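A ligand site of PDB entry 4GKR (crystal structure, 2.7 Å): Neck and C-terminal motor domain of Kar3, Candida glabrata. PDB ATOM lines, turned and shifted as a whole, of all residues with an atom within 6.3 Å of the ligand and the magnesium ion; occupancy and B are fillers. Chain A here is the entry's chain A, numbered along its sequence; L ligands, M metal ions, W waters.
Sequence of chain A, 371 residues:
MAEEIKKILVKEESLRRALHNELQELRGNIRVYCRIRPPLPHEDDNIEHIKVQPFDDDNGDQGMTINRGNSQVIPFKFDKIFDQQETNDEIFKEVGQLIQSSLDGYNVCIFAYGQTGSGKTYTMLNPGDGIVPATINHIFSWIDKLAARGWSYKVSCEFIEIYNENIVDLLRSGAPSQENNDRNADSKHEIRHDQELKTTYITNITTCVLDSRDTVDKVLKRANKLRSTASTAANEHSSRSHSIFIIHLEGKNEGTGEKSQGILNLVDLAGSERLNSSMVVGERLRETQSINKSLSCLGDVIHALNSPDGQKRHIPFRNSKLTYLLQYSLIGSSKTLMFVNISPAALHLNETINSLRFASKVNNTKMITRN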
ATOM      1  N   ARG A  35     -30.926   6.425  18.551  1.00  0.00           N
ATOM      2  CA  ARG A  35     -29.466   6.463  18.407  1.00  0.00           C
ATOM      3  C   ARG A  35     -28.952   5.428  17.429  1.00  0.00           C
ATOM      4  O   ARG A  35     -29.151   4.235  17.624  1.00  0.00           O
ATOM      5  CB  ARG A  35     -28.767   6.272  19.762  1.00  0.00           C
ATOM      6  CG  ARG A  35     -27.254   6.125  19.621  1.00  0.00           C
ATOM      7  CD  ARG A  35     -26.541   5.987  20.949  1.00  0.00           C
ATOM      8  NE  ARG A  35     -25.197   6.542  20.876  1.00  0.00           N
ATOM      9  CZ  ARG A  35     -24.295   6.483  21.860  1.00  0.00           C
ATOM     10  NH1 ARG A  35     -24.580   5.894  23.021  1.00  0.00           N
ATOM     11  NH2 ARG A  35     -23.108   7.023  21.684  1.00  0.00           N
ATOM     12  N   ILE A  36     -28.259   5.881  16.390  1.00  0.00           N
ATOM     13  CA  ILE A  36     -27.618   4.941  15.479  1.00  0.00           C
ATOM     14  C   ILE A  36     -26.198   4.705  15.963  1.00  0.00           C
ATOM     15  O   ILE A  36     -25.429   5.634  16.077  1.00  0.00           O
ATOM     16  CB  ILE A  36     -27.584   5.500  14.032  1.00  0.00           C
ATOM     17  CG1 ILE A  36     -29.005   5.825  13.572  1.00  0.00           C
ATOM     18  CG2 ILE A  36     -26.934   4.501  13.078  1.00  0.00           C
ATOM     19  CD1 ILE A  36     -29.094   6.682  12.336  1.00  0.00           C
ATOM     20  N   ARG A  37     -25.839   3.466  16.275  1.00  0.00           N
ATOM     21  CA  ARG A  37     -24.429   3.176  16.597  1.00  0.00           C
ATOM     22  C   ARG A  37     -23.541   3.148  15.339  1.00  0.00           C
ATOM     23  O   ARG A  37     -24.023   2.932  14.230  1.00  0.00           O
ATOM     24  CB  ARG A  37     -24.275   1.872  17.373  1.00  0.00           C
ATOM     25  CG  ARG A  37     -24.533   0.612  16.563  1.00  0.00           C
ATOM     26  CD  ARG A  37     -23.923  -0.600  17.221  1.00  0.00           C
ATOM     27  NE  ARG A  37     -24.318  -1.843  16.569  1.00  0.00           N
ATOM     28  CZ  ARG A  37     -23.853  -2.291  15.406  1.00  0.00           C
ATOM     29  NH1 ARG A  37     -22.968  -1.586  14.721  1.00  0.00           N
ATOM     30  NH2 ARG A  37     -24.293  -3.445  14.927  1.00  0.00           N
ATOM     31  N   PRO A  38     -22.225   3.397  15.513  1.00  0.00           N
ATOM     32  CA  PRO A  38     -21.249   3.201  14.430  1.00  0.00           C
ATOM     33  C   PRO A  38     -21.190   1.755  13.967  1.00  0.00           C
ATOM     34  O   PRO A  38     -21.549   0.861  14.732  1.00  0.00           O
ATOM     35  CB  PRO A  38     -19.911   3.595  15.060  1.00  0.00           C
ATOM     36  CG  PRO A  38     -20.182   3.722  16.523  1.00  0.00           C
ATOM     37  CD  PRO A  38     -21.618   4.059  16.684  1.00  0.00           C
ATOM     38  N   LEU A  40     -19.600  -1.953  13.100  1.00  0.00           N
ATOM     39  CA  LEU A  40     -18.571  -2.798  13.711  1.00  0.00           C
ATOM     40  C   LEU A  40     -17.546  -3.230  12.639  1.00  0.00           C
ATOM     41  O   LEU A  40     -17.867  -3.190  11.454  1.00  0.00           O
ATOM     42  CB  LEU A  40     -19.201  -4.016  14.408  1.00  0.00           C
ATOM     43  CG  LEU A  40     -20.041  -3.730  15.668  1.00  0.00           C
ATOM     44  CD1 LEU A  40     -21.004  -4.871  15.952  1.00  0.00           C
ATOM     45  CD2 LEU A  40     -19.179  -3.430  16.887  1.00  0.00           C
ATOM     46  N   GLN A  84     -24.142   8.532  14.074  1.00  0.00           N
ATOM     47  CA  GLN A  84     -23.070   7.620  14.483  1.00  0.00           C
ATOM     48  C   GLN A  84     -21.869   8.287  15.173  1.00  0.00           C
ATOM     49  O   GLN A  84     -21.107   7.627  15.868  1.00  0.00           O
ATOM     50  CB  GLN A  84     -22.563   6.836  13.285  1.00  0.00           C
ATOM     51  CG  GLN A  84     -23.661   6.354  12.365  1.00  0.00           C
ATOM     52  CD  GLN A  84     -23.123   5.468  11.284  1.00  0.00           C
ATOM     53  OE1 GLN A  84     -22.341   5.894  10.435  1.00  0.00           O
ATOM     54  NE2 GLN A  84     -23.521   4.206  11.312  1.00  0.00           N
ATOM     55  N   GLU A  86     -22.078  10.699  17.418  1.00  0.00           N
ATOM     56  CA  GLU A  86     -22.431  11.184  18.754  1.00  0.00           C
ATOM     57  C   GLU A  86     -22.012  10.211  19.870  1.00  0.00           C
ATOM     58  O   GLU A  86     -22.285   9.009  19.813  1.00  0.00           O
ATOM     59  CB  GLU A  86     -23.910  11.549  18.845  1.00  0.00           C
ATOM     60  N   ASN A  88     -21.368   9.047  24.085  1.00  0.00           N
ATOM     61  CA  ASN A  88     -22.083   8.975  25.361  1.00  0.00           C
ATOM     62  C   ASN A  88     -22.114  10.301  26.109  1.00  0.00           C
ATOM     63  O   ASN A  88     -23.142  10.683  26.669  1.00  0.00           O
ATOM     64  CB  ASN A  88     -21.483   7.883  26.254  1.00  0.00           C
ATOM     65  CG  ASN A  88     -22.009   6.499  25.924  1.00  0.00           C
ATOM     66  OD1 ASN A  88     -22.825   6.334  25.012  1.00  0.00           O
ATOM     67  ND2 ASN A  88     -21.571   5.514  26.669  1.00  0.00           N
ATOM     68  N   GLY A 114     -34.292  -1.982  21.598  1.00  0.00           N
ATOM     69  CA  GLY A 114     -33.799  -2.298  20.261  1.00  0.00           C
ATOM     70  C   GLY A 114     -33.173  -3.680  20.201  1.00  0.00           C
ATOM     71  O   GLY A 114     -33.078  -4.376  21.213  1.00  0.00           O
ATOM     72  N   GLN A 115     -32.743  -4.081  19.010  1.00  0.00           N
ATOM     73  CA  GLN A 115     -32.285  -5.457  18.817  1.00  0.00           C
ATOM     74  C   GLN A 115     -30.970  -5.787  19.536  1.00  0.00           C
ATOM     75  O   GLN A 115     -30.178  -4.912  19.808  1.00  0.00           O
ATOM     76  CB  GLN A 115     -32.208  -5.809  17.331  1.00  0.00           C
ATOM     77  CG  GLN A 115     -31.173  -5.071  16.520  1.00  0.00           C
ATOM     78  CD  GLN A 115     -31.025  -5.680  15.134  1.00  0.00           C
ATOM     79  OE1 GLN A 115     -30.941  -4.963  14.146  1.00  0.00           O
ATOM     80  NE2 GLN A 115     -31.000  -7.006  15.077  1.00  0.00           N
ATOM     81  N   THR A 116     -30.767  -7.065  19.843  1.00  0.00           N
ATOM     82  CA  THR A 116     -29.495  -7.502  20.366  1.00  0.00           C
ATOM     83  C   THR A 116     -28.437  -7.075  19.342  1.00  0.00           C
ATOM     84  O   THR A 116     -28.605  -7.288  18.138  1.00  0.00           O
ATOM     85  CB  THR A 116     -29.493  -9.014  20.590  1.00  0.00           C
ATOM     86  OG1 THR A 116     -30.435  -9.327  21.632  1.00  0.00           O
ATOM     87  CG2 THR A 116     -28.118  -9.524  20.982  1.00  0.00           C
ATOM     88  N   GLY A 117     -27.380  -6.417  19.819  1.00  0.00           N
ATOM     89  CA  GLY A 117     -26.359  -5.880  18.949  1.00  0.00           C
ATOM     90  C   GLY A 117     -26.468  -4.389  18.663  1.00  0.00           C
ATOM     91  O   GLY A 117     -25.558  -3.816  18.063  1.00  0.00           O
ATOM     92  N   SER A 118     -27.545  -3.744  19.063  1.00  0.00           N
ATOM     93  CA  SER A 118     -27.726  -2.366  18.620  1.00  0.00           C
ATOM     94  C   SER A 118     -27.093  -1.305  19.518  1.00  0.00           C
ATOM     95  O   SER A 118     -27.058  -0.135  19.140  1.00  0.00           O
ATOM     96  CB  SER A 118     -29.189  -2.077  18.417  1.00  0.00           C
ATOM     97  OG  SER A 118     -29.876  -2.205  19.651  1.00  0.00           O
ATOM     98  N   GLY A 119     -26.595  -1.705  20.690  1.00  0.00           N
ATOM     99  CA  GLY A 119     -25.957  -0.766  21.603  1.00  0.00           C
ATOM    100  C   GLY A 119     -26.725  -0.329  22.861  1.00  0.00           C
ATOM    101  O   GLY A 119     -26.479   0.759  23.393  1.00  0.00           O
ATOM    102  N   LYS A 120     -27.629  -1.169  23.349  1.00  0.00           N
ATOM    103  CA  LYS A 120     -28.383  -0.840  24.552  1.00  0.00           C
ATOM    104  C   LYS A 120     -27.486  -0.819  25.790  1.00  0.00           C
ATOM    105  O   LYS A 120     -27.482   0.148  26.553  1.00  0.00           O
ATOM    106  CB  LYS A 120     -29.513  -1.838  24.769  1.00  0.00           C
ATOM    107  CG  LYS A 120     -30.564  -1.864  23.689  1.00  0.00           C
ATOM    108  CD  LYS A 120     -31.673  -2.827  24.078  1.00  0.00           C
ATOM    109  CE  LYS A 120     -31.200  -4.281  24.093  1.00  0.00           C
ATOM    110  NZ  LYS A 120     -30.596  -4.685  22.794  1.00  0.00           N
ATOM    111  N   THR A 121     -26.692  -1.888  25.977  1.00  0.00           N
ATOM    112  CA  THR A 121     -25.818  -1.988  27.128  1.00  0.00           C
ATOM    113  C   THR A 121     -24.786  -0.877  27.075  1.00  0.00           C
ATOM    114  O   THR A 121     -24.440  -0.282  28.098  1.00  0.00           O
ATOM    115  CB  THR A 121     -25.125  -3.355  27.160  1.00  0.00           C
ATOM    116  OG1 THR A 121     -26.117  -4.391  27.268  1.00  0.00           O
ATOM    117  CG2 THR A 121     -24.179  -3.477  28.352  1.00  0.00           C
ATOM    118  N   TYR A 122     -24.300  -0.595  25.884  1.00  0.00           N
ATOM    119  CA  TYR A 122     -23.282   0.407  25.715  1.00  0.00           C
ATOM    120  C   TYR A 122     -23.844   1.773  26.106  1.00  0.00           C
ATOM    121  O   TYR A 122     -23.199   2.530  26.821  1.00  0.00           O
ATOM    122  CB  TYR A 122     -22.766   0.411  24.272  1.00  0.00           C
ATOM    123  CG  TYR A 122     -21.722   1.460  24.026  1.00  0.00           C
ATOM    124  CD1 TYR A 122     -22.090   2.768  23.717  1.00  0.00           C
ATOM    125  CD2 TYR A 122     -20.356   1.153  24.116  1.00  0.00           C
ATOM    126  CE1 TYR A 122     -21.139   3.754  23.506  1.00  0.00           C
ATOM    127  CE2 TYR A 122     -19.383   2.122  23.895  1.00  0.00           C
ATOM    128  CZ  TYR A 122     -19.790   3.425  23.585  1.00  0.00           C
ATOM    129  OH  TYR A 122     -18.858   4.399  23.363  1.00  0.00           O
ATOM    130  N   THR A 123     -25.052   2.084  25.648  1.00  0.00           N
ATOM    131  CA  THR A 123     -25.725   3.295  26.030  1.00  0.00           C
ATOM    132  C   THR A 123     -25.964   3.404  27.543  1.00  0.00           C
ATOM    133  O   THR A 123     -25.716   4.459  28.124  1.00  0.00           O
ATOM    134  CB  THR A 123     -27.066   3.431  25.273  1.00  0.00           C
ATOM    135  OG1 THR A 123     -26.798   3.553  23.881  1.00  0.00           O
ATOM    136  CG2 THR A 123     -27.847   4.685  25.735  1.00  0.00           C
ATOM    137  N   ASN A 126     -21.828   1.750  29.793  1.00  0.00           N
ATOM    138  CA  ASN A 126     -20.431   1.930  29.445  1.00  0.00           C
ATOM    139  C   ASN A 126     -19.650   2.657  30.561  1.00  0.00           C
ATOM    140  O   ASN A 126     -20.075   3.725  31.001  1.00  0.00           O
ATOM    141  CB  ASN A 126     -20.326   2.694  28.138  1.00  0.00           C
ATOM    142  CG  ASN A 126     -18.996   2.506  27.452  1.00  0.00           C
ATOM    143  OD1 ASN A 126     -18.323   3.472  27.116  1.00  0.00           O
ATOM    144  ND2 ASN A 126     -18.593   1.243  27.273  1.00  0.00           N
ATOM    145  N   SER A 238     -28.120 -12.462  29.252  1.00  0.00           N
ATOM    146  CA  SER A 238     -28.471 -11.077  29.567  1.00  0.00           C
ATOM    147  C   SER A 238     -29.110 -10.351  28.387  1.00  0.00           C
ATOM    148  O   SER A 238     -29.848  -9.393  28.577  1.00  0.00           O
ATOM    149  CB  SER A 238     -27.287 -10.327  30.131  1.00  0.00           C
ATOM    150  OG  SER A 238     -26.294 -10.353  29.166  1.00  0.00           O
ATOM    151  N   SER A 239     -28.843 -10.812  27.170  1.00  0.00           N
ATOM    152  CA  SER A 239     -29.477 -10.207  26.004  1.00  0.00           C
ATOM    153  C   SER A 239     -30.957 -10.598  25.862  1.00  0.00           C
ATOM    154  O   SER A 239     -31.699 -10.003  25.074  1.00  0.00           O
ATOM    155  CB  SER A 239     -28.709 -10.562  24.740  1.00  0.00           C
ATOM    156  OG  SER A 239     -29.211 -11.784  24.238  1.00  0.00           O
ATOM    157  N   ASP A 268     -32.396  -1.312  30.800  1.00  0.00           N
ATOM    158  CA  ASP A 268     -31.727  -1.855  29.626  1.00  0.00           C
ATOM    159  C   ASP A 268     -32.575  -3.074  29.238  1.00  0.00           C
ATOM    160  O   ASP A 268     -32.459  -4.115  29.875  1.00  0.00           O
ATOM    161  CB  ASP A 268     -30.289  -2.227  30.055  1.00  0.00           C
ATOM    162  CG  ASP A 268     -29.510  -3.033  28.992  1.00  0.00           C
ATOM    163  OD1 ASP A 268     -29.975  -3.134  27.838  1.00  0.00           O
ATOM    164  OD2 ASP A 268     -28.393  -3.562  29.318  1.00  0.00           O
ATOM    165  N   LEU A 269     -33.422  -2.967  28.237  1.00  0.00           N
ATOM    166  CA  LEU A 269     -34.425  -4.010  27.964  1.00  0.00           C
ATOM    167  C   LEU A 269     -33.900  -5.267  27.277  1.00  0.00           C
ATOM    168  O   LEU A 269     -32.808  -5.278  26.704  1.00  0.00           O
ATOM    169  CB  LEU A 269     -35.609  -3.430  27.188  1.00  0.00           C
ATOM    170  CG  LEU A 269     -36.488  -2.412  27.939  1.00  0.00           C
ATOM    171  CD1 LEU A 269     -37.408  -1.581  27.039  1.00  0.00           C
ATOM    172  CD2 LEU A 269     -37.327  -3.076  29.017  1.00  0.00           C
ATOM    173  N   ASN A 341     -32.321   2.130  20.100  1.00  0.00           N
ATOM    174  CA  ASN A 341     -31.008   1.884  19.551  1.00  0.00           C
ATOM    175  C   ASN A 341     -31.178   1.141  18.234  1.00  0.00           C
ATOM    176  O   ASN A 341     -31.889   0.136  18.188  1.00  0.00           O
ATOM    177  CB  ASN A 341     -30.154   1.082  20.542  1.00  0.00           C
ATOM    178  CG  ASN A 341     -29.837   1.866  21.803  1.00  0.00           C
ATOM    179  OD1 ASN A 341     -30.576   1.794  22.778  1.00  0.00           O
ATOM    180  ND2 ASN A 341     -28.763   2.637  21.785  1.00  0.00           N
HETATM  181  P1  LIG L   1     -26.936  -4.636  22.938  1.00  0.00           P
HETATM  182  O1  LIG L   1     -27.905  -3.633  22.345  1.00  0.00           O
HETATM  183  O2  LIG L   1     -26.725  -4.500  24.420  1.00  0.00           O
HETATM  184  O3  LIG L   1     -27.227  -6.013  22.433  1.00  0.00           O
HETATM  185  P2  LIG L   1     -24.168  -3.738  23.035  1.00  0.00           P
HETATM  186  O4  LIG L   1     -24.261  -2.482  23.840  1.00  0.00           O
HETATM  187  O5  LIG L   1     -23.555  -4.968  23.662  1.00  0.00           O
HETATM  188  O6  LIG L   1     -25.538  -4.171  22.282  1.00  0.00           O
HETATM  189  O7  LIG L   1     -23.337  -3.217  21.761  1.00  0.00           O
HETATM  190  C1  LIG L   1     -23.013  -4.079  20.667  1.00  0.00           C
HETATM  191  C2  LIG L   1     -21.563  -3.829  20.232  1.00  0.00           C
HETATM  192  O8  LIG L   1     -21.391  -2.578  19.530  1.00  0.00           O
HETATM  193  C3  LIG L   1     -20.641  -3.763  21.422  1.00  0.00           C
HETATM  194  O9  LIG L   1     -19.459  -4.435  21.023  1.00  0.00           O
HETATM  195  C4  LIG L   1     -20.378  -2.266  21.633  1.00  0.00           C
HETATM  196  O10 LIG L   1     -19.087  -1.964  22.149  1.00  0.00           O
HETATM  197  C5  LIG L   1     -20.553  -1.666  20.255  1.00  0.00           C
HETATM  198  N1  LIG L   1     -21.249  -0.374  20.319  1.00  0.00           N
HETATM  199  C6  LIG L   1     -22.564  -0.213  20.504  1.00  0.00           C
HETATM  200  N2  LIG L   1     -22.928   1.093  20.495  1.00  0.00           N
HETATM  201  C7  LIG L   1     -21.822   1.805  20.295  1.00  0.00           C
HETATM  202  C8  LIG L   1     -21.495   3.243  20.174  1.00  0.00           C
HETATM  203  N3  LIG L   1     -22.460   4.177  20.268  1.00  0.00           N
HETATM  204  N4  LIG L   1     -20.201   3.575  19.970  1.00  0.00           N
HETATM  205  C9  LIG L   1     -19.226   2.642  19.876  1.00  0.00           C
HETATM  206  N5  LIG L   1     -19.446   1.319  19.974  1.00  0.00           N
HETATM  207  C10 LIG L   1     -20.702   0.841  20.182  1.00  0.00           C
HETATM  208 MG    MG M   1     -27.042  -5.944  25.923  1.00  0.00          MG
HETATM  209  O   HOH W   1     -30.070  -7.302  23.739  1.00  0.00           O
HETATM  210  O   HOH W   2     -25.022  -6.081  25.611  1.00  0.00           O
HETATM  211  O   HOH W   3     -26.656  -7.074  27.561  1.00  0.00           O
HETATM  212  O   HOH W   4     -27.385  -7.270  24.757  1.00  0.00           O
HETATM  213  O   HOH W   5     -28.684  -5.216  26.738  1.00  0.00           O
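The backbone NH (N) of Ser 118 sits at hydrogen-bond distance from an oxygen (O1) of the ligand (3.3 Å).
The side-chain amino group (NZ) of Lys 120 is in salt-bridge range of an oxygen (O1) of the ligand, 2.9 Å away.
An oxygen (O1) of the ligand sits at hydrogen-bond distance from the backbone NH (N) of Lys 120 (2.7 Å).
N of Thr 121 lies within hydrogen-bond range of O4 of the ligand (3.3 Å).
The backbone NH of Tyr 122 lies within hydrogen-bond range of an oxygen (O4) of the ligand (2.8 Å).
N of Gly 119 sits at hydrogen-bond distance from O1 of the ligand.
The backbone NH of Gly 117 lies within hydrogen-bond range of an oxygen (O3) of the ligand.
OD1 of Asn 88 is in hydrogen-bond range of NH1 of Arg 35, at 2.7 Å.
O of Asn 341 lies within hydrogen-bond range of OG of Ser 118 (3.4 Å).
The guanidinium group (NE) of Arg 37 is in hydrogen-bond range of the backbone carbonyl oxygen (O) of Gly 117 (2.8 Å).
The backbone carbonyl oxygen (O) of Gln 115 is in hydrogen-bond range of the side-chain hydroxyl (OG) of Ser 118, 2.7 Å away.
The backbone carbonyl oxygen of Arg 37 lies within hydrogen-bond range of the side-chain amide nitrogen of Gln 84.
The side-chain amide nitrogen (ND2) of Asn 341 lies within hydrogen-bond range of the backbone carbonyl oxygen (O) of Gly 119 (3.4 Å).
OG1 of Thr 121 lies close to OD2 of Asp 268 (3.2 Å).
NZ of Lys 120 sits at hydrogen-bond distance from O of Gly 114 (3.0 Å).
A nitrogen (N3) of the ligand sits close to the guanidinium group (NH2) of Arg 35, 3.2 Å away.
Arg 37 touches the ligand.
Pro 38 touches the ligand.
Leu 40 touches the ligand (CD2 to O8, 3.6 Å).
Gln 115 touches the ligand (O to O1, 3.6 Å).
Thr 116 touches the ligand.
One residue has an atom within 4 Å of the magnesium ion: Thr 121.
The nearest printed residue that does not touch the magnesium ion is Asp 268 (4.4 Å).
The magnesium ion is bound by water W4, water W5, water W3, water W2, an oxygen (O2) of the ligand and the side-chain hydroxyl of Thr 121.
Water W1 lies within hydrogen-bond range of the side-chain amino group of Lys 120 (2.8 Å), the side-chain hydroxyl of Thr 116 (2.9 Å), an oxygen (O3) of the ligand (3.4 Å) and the backbone carbonyl oxygen of Ser 239 (3.4 Å).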
